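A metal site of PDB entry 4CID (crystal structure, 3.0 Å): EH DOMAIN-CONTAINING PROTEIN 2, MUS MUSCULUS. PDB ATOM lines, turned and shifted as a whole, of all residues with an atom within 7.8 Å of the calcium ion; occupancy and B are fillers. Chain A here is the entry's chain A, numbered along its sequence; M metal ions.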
ATOM      1  N   LYS A 473     -35.168   2.401 -31.108  1.00  0.00           N
ATOM      2  CA  LYS A 473     -33.961   2.441 -30.308  1.00  0.00           C
ATOM      3  C   LYS A 473     -32.762   2.000 -31.141  1.00  0.00           C
ATOM      4  O   LYS A 473     -32.756   0.911 -31.707  1.00  0.00           O
ATOM      5  CB  LYS A 473     -34.100   1.552 -29.084  1.00  0.00           C
ATOM      6  CG  LYS A 473     -35.008   2.148 -28.021  1.00  0.00           C
ATOM      7  CD  LYS A 473     -35.169   1.230 -26.818  1.00  0.00           C
ATOM      8  CE  LYS A 473     -36.048   1.854 -25.755  1.00  0.00           C
ATOM      9  NZ  LYS A 473     -35.355   2.944 -25.000  1.00  0.00           N
ATOM     10  N   LEU A 474     -31.768   2.881 -31.208  1.00  0.00           N
ATOM     11  CA  LEU A 474     -30.534   2.593 -31.892  1.00  0.00           C
ATOM     12  C   LEU A 474     -29.552   1.955 -30.919  1.00  0.00           C
ATOM     13  O   LEU A 474     -29.372   2.435 -29.800  1.00  0.00           O
ATOM     14  CB  LEU A 474     -29.920   3.869 -32.468  1.00  0.00           C
ATOM     15  CG  LEU A 474     -28.642   3.704 -33.295  1.00  0.00           C
ATOM     16  CD1 LEU A 474     -28.895   2.817 -34.499  1.00  0.00           C
ATOM     17  CD2 LEU A 474     -28.095   5.061 -33.718  1.00  0.00           C
ATOM     18  N   TRP A 497     -21.541  10.523 -25.682  1.00  0.00           N
ATOM     19  CA  TRP A 497     -22.370   9.351 -25.388  1.00  0.00           C
ATOM     20  C   TRP A 497     -22.891   9.379 -23.953  1.00  0.00           C
ATOM     21  O   TRP A 497     -24.111   9.249 -23.722  1.00  0.00           O
ATOM     22  CB  TRP A 497     -21.596   8.051 -25.593  1.00  0.00           C
ATOM     23  CG  TRP A 497     -22.403   6.891 -25.171  1.00  0.00           C
ATOM     24  CD1 TRP A 497     -22.425   6.322 -23.942  1.00  0.00           C
ATOM     25  CD2 TRP A 497     -23.379   6.207 -25.948  1.00  0.00           C
ATOM     26  NE1 TRP A 497     -23.331   5.287 -23.910  1.00  0.00           N
ATOM     27  CE2 TRP A 497     -23.934   5.195 -25.134  1.00  0.00           C
ATOM     28  CE3 TRP A 497     -23.831   6.324 -27.277  1.00  0.00           C
ATOM     29  CZ2 TRP A 497     -24.908   4.318 -25.595  1.00  0.00           C
ATOM     30  CZ3 TRP A 497     -24.810   5.452 -27.725  1.00  0.00           C
ATOM     31  CH2 TRP A 497     -25.331   4.461 -26.890  1.00  0.00           C
ATOM     32  N   SER A 500     -25.587  11.958 -23.700  1.00  0.00           N
ATOM     33  CA  SER A 500     -26.759  11.643 -24.497  1.00  0.00           C
ATOM     34  C   SER A 500     -27.568  10.443 -23.991  1.00  0.00           C
ATOM     35  O   SER A 500     -28.794  10.470 -24.050  1.00  0.00           O
ATOM     36  CB  SER A 500     -26.352  11.411 -25.943  1.00  0.00           C
ATOM     37  OG  SER A 500     -25.742  12.575 -26.476  1.00  0.00           O
ATOM     38  N   ASP A 501     -26.904   9.389 -23.524  1.00  0.00           N
ATOM     39  CA  ASP A 501     -27.658   8.235 -23.037  1.00  0.00           C
ATOM     40  C   ASP A 501     -28.251   8.543 -21.658  1.00  0.00           C
ATOM     41  O   ASP A 501     -27.753   8.071 -20.635  1.00  0.00           O
ATOM     42  CB  ASP A 501     -26.799   6.973 -22.990  1.00  0.00           C
ATOM     43  CG  ASP A 501     -27.619   5.706 -22.732  1.00  0.00           C
ATOM     44  OD1 ASP A 501     -28.869   5.777 -22.727  1.00  0.00           O
ATOM     45  OD2 ASP A 501     -27.006   4.640 -22.529  1.00  0.00           O
ATOM     46  N   VAL A 502     -29.344   9.305 -21.651  1.00  0.00           N
ATOM     47  CA  VAL A 502     -29.923   9.829 -20.410  1.00  0.00           C
ATOM     48  C   VAL A 502     -30.515   8.720 -19.553  1.00  0.00           C
ATOM     49  O   VAL A 502     -30.282   8.676 -18.349  1.00  0.00           O
ATOM     50  CB  VAL A 502     -31.004  10.889 -20.695  1.00  0.00           C
ATOM     51  CG1 VAL A 502     -31.663  11.338 -19.410  1.00  0.00           C
ATOM     52  CG2 VAL A 502     -30.391  12.082 -21.409  1.00  0.00           C
ATOM     53  N   ASP A 503     -31.282   7.814 -20.160  1.00  0.00           N
ATOM     54  CA  ASP A 503     -31.859   6.692 -19.410  1.00  0.00           C
ATOM     55  C   ASP A 503     -30.841   5.568 -19.142  1.00  0.00           C
ATOM     56  O   ASP A 503     -31.160   4.593 -18.454  1.00  0.00           O
ATOM     57  CB  ASP A 503     -33.128   6.159 -20.105  1.00  0.00           C
ATOM     58  CG  ASP A 503     -32.850   5.514 -21.457  1.00  0.00           C
ATOM     59  OD1 ASP A 503     -31.798   5.791 -22.063  1.00  0.00           O
ATOM     60  OD2 ASP A 503     -33.705   4.724 -21.921  1.00  0.00           O
ATOM     61  N   ARG A 504     -29.627   5.743 -19.665  1.00  0.00           N
ATOM     62  CA  ARG A 504     -28.478   4.854 -19.446  1.00  0.00           C
ATOM     63  C   ARG A 504     -28.818   3.368 -19.607  1.00  0.00           C
ATOM     64  O   ARG A 504     -28.536   2.551 -18.732  1.00  0.00           O
ATOM     65  CB  ARG A 504     -27.758   5.164 -18.121  1.00  0.00           C
ATOM     66  CG  ARG A 504     -28.623   5.554 -16.935  1.00  0.00           C
ATOM     67  CD  ARG A 504     -27.771   6.030 -15.777  1.00  0.00           C
ATOM     68  NE  ARG A 504     -28.578   6.580 -14.687  1.00  0.00           N
ATOM     69  CZ  ARG A 504     -29.213   5.851 -13.768  1.00  0.00           C
ATOM     70  NH1 ARG A 504     -29.149   4.518 -13.785  1.00  0.00           N
ATOM     71  NH2 ARG A 504     -29.918   6.458 -12.819  1.00  0.00           N
ATOM     72  N   ASP A 505     -29.403   3.041 -20.753  1.00  0.00           N
ATOM     73  CA  ASP A 505     -29.744   1.668 -21.110  1.00  0.00           C
ATOM     74  C   ASP A 505     -28.817   1.106 -22.208  1.00  0.00           C
ATOM     75  O   ASP A 505     -28.989  -0.038 -22.631  1.00  0.00           O
ATOM     76  CB  ASP A 505     -31.203   1.575 -21.563  1.00  0.00           C
ATOM     77  CG  ASP A 505     -31.442   2.187 -22.944  1.00  0.00           C
ATOM     78  OD1 ASP A 505     -30.830   3.232 -23.247  1.00  0.00           O
ATOM     79  OD2 ASP A 505     -32.252   1.630 -23.714  1.00  0.00           O
ATOM     80  N   GLY A 506     -27.871   1.909 -22.667  1.00  0.00           N
ATOM     81  CA  GLY A 506     -26.910   1.472 -23.678  1.00  0.00           C
ATOM     82  C   GLY A 506     -27.377   1.645 -25.109  1.00  0.00           C
ATOM     83  O   GLY A 506     -26.695   1.229 -26.043  1.00  0.00           O
ATOM     84  N   MET A 507     -28.528   2.288 -25.285  1.00  0.00           N
ATOM     85  CA  MET A 507     -29.091   2.544 -26.604  1.00  0.00           C
ATOM     86  C   MET A 507     -29.489   3.980 -26.692  1.00  0.00           C
ATOM     87  O   MET A 507     -29.528   4.682 -25.676  1.00  0.00           O
ATOM     88  CB  MET A 507     -30.308   1.659 -26.762  1.00  0.00           C
ATOM     89  CG  MET A 507     -29.971   0.181 -26.667  1.00  0.00           C
ATOM     90  SD  MET A 507     -31.562  -0.876 -27.157  1.00  0.00           S
ATOM     91  CE  MET A 507     -31.871  -1.736 -25.404  1.00  0.00           C
ATOM     92  N   LEU A 508     -29.804   4.444 -27.892  1.00  0.00           N
ATOM     93  CA  LEU A 508     -30.299   5.826 -28.057  1.00  0.00           C
ATOM     94  C   LEU A 508     -31.624   5.844 -28.799  1.00  0.00           C
ATOM     95  O   LEU A 508     -31.710   5.364 -29.917  1.00  0.00           O
ATOM     96  CB  LEU A 508     -29.286   6.681 -28.808  1.00  0.00           C
ATOM     97  CG  LEU A 508     -27.928   6.871 -28.132  1.00  0.00           C
ATOM     98  CD1 LEU A 508     -26.948   7.509 -29.113  1.00  0.00           C
ATOM     99  CD2 LEU A 508     -28.054   7.726 -26.885  1.00  0.00           C
ATOM    100  N   ASP A 509     -32.655   6.409 -28.170  1.00  0.00           N
ATOM    101  CA  ASP A 509     -33.913   6.681 -28.864  1.00  0.00           C
ATOM    102  C   ASP A 509     -33.796   8.010 -29.615  1.00  0.00           C
ATOM    103  O   ASP A 509     -32.790   8.718 -29.503  1.00  0.00           O
ATOM    104  CB  ASP A 509     -35.095   6.676 -27.892  1.00  0.00           C
ATOM    105  CG  ASP A 509     -35.027   7.809 -26.874  1.00  0.00           C
ATOM    106  OD1 ASP A 509     -34.596   8.938 -27.229  1.00  0.00           O
ATOM    107  OD2 ASP A 509     -35.425   7.566 -25.714  1.00  0.00           O
ATOM    108  N   GLU A 512     -32.687  11.178 -27.584  1.00  0.00           N
ATOM    109  CA  GLU A 512     -31.290  11.049 -27.172  1.00  0.00           C
ATOM    110  C   GLU A 512     -30.365  11.212 -28.374  1.00  0.00           C
ATOM    111  O   GLU A 512     -29.311  11.854 -28.261  1.00  0.00           O
ATOM    112  CB  GLU A 512     -31.050   9.701 -26.510  1.00  0.00           C
ATOM    113  CG  GLU A 512     -31.727   9.539 -25.159  1.00  0.00           C
ATOM    114  CD  GLU A 512     -31.500   8.180 -24.553  1.00  0.00           C
ATOM    115  OE1 GLU A 512     -31.818   7.160 -25.217  1.00  0.00           O
ATOM    116  OE2 GLU A 512     -31.003   8.104 -23.412  1.00  0.00           O
ATOM    117  N   PHE A 513     -30.764  10.641 -29.507  1.00  0.00           N
ATOM    118  CA  PHE A 513     -29.996  10.781 -30.740  1.00  0.00           C
ATOM    119  C   PHE A 513     -29.947  12.243 -31.182  1.00  0.00           C
ATOM    120  O   PHE A 513     -28.879  12.767 -31.513  1.00  0.00           O
ATOM    121  CB  PHE A 513     -30.584   9.920 -31.857  1.00  0.00           C
ATOM    122  CG  PHE A 513     -29.764   9.925 -33.113  1.00  0.00           C
ATOM    123  CD1 PHE A 513     -28.652   9.105 -33.228  1.00  0.00           C
ATOM    124  CD2 PHE A 513     -30.098  10.766 -34.163  1.00  0.00           C
ATOM    125  CE1 PHE A 513     -27.886   9.106 -34.383  1.00  0.00           C
ATOM    126  CE2 PHE A 513     -29.329  10.773 -35.327  1.00  0.00           C
ATOM    127  CZ  PHE A 513     -28.231   9.942 -35.428  1.00  0.00           C
ATOM    128  N   LYS A 542     -38.138  13.175 -20.742  1.00  0.00           N
ATOM    129  CA  LYS A 542     -37.276  12.469 -19.804  1.00  0.00           C
ATOM    130  C   LYS A 542     -37.090  13.217 -18.482  1.00  0.00           C
ATOM    131  O   LYS A 542     -36.730  12.597 -17.481  1.00  0.00           O
ATOM    132  CB  LYS A 542     -35.902  12.225 -20.414  1.00  0.00           C
ATOM    133  CG  LYS A 542     -35.915  11.559 -21.774  1.00  0.00           C
ATOM    134  CD  LYS A 542     -36.379  10.119 -21.687  1.00  0.00           C
ATOM    135  CE  LYS A 542     -36.387   9.476 -23.069  1.00  0.00           C
ATOM    136  NZ  LYS A 542     -35.036   9.527 -23.691  1.00  0.00           N
HETATM  137 CA    CA M   1     -31.011   5.305 -24.171  1.00  0.00          CA
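Merely in contact with the calcium ion: Leu 508 (3.98 Å).
Of the 16 residues printed, 6 come within 4 Å of the calcium ion.
The nearest printed residue that does not touch the calcium ion is Asp 509 (4.5 Å).
The side-chain amino group of Lys 473 is in salt-bridge range of the side-chain carboxylate of Asp 505, 3.6 Å away.
The side-chain carboxylate of Asp 509 lies within hydrogen-bond range of the backbone NH of Glu 512 (3.0 Å).
The side-chain carboxylate (OE2) of Glu 512 is in hydrogen-bond range of the backbone NH (N) of Val 502, 2.7 Å away.
The side-chain carboxylate (OD2) of Asp 503 is in salt-bridge range of the side-chain amino group (NZ) of Lys 473 (3.9 Å).
The side-chain carboxylate (OD1) of Asp 501 sits close to the backbone NH (N) of Arg 504, 3.2 Å away.
N of Gly 506 lies within hydrogen-bond range of OD2 of Asp 501 (2.9 Å).
The backbone carbonyl oxygen (O) of Leu 508 is in hydrogen-bond range of the backbone NH (N) of Leu 474 (2.8 Å).
The calcium ion is bound by O of Met 507 (2.2 Å), OD1 of Asp 505 (2.3 Å), OE1 of Glu 512 (2.3 Å), OD1 of Asp 503 (2.3 Å) and OD1 of Asp 501 (2.6 Å).
The calcium ion has five donor atoms within binding distance.
Slightly farther from the calcium ion lies OE2 of Glu 512 (2.9 Å).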
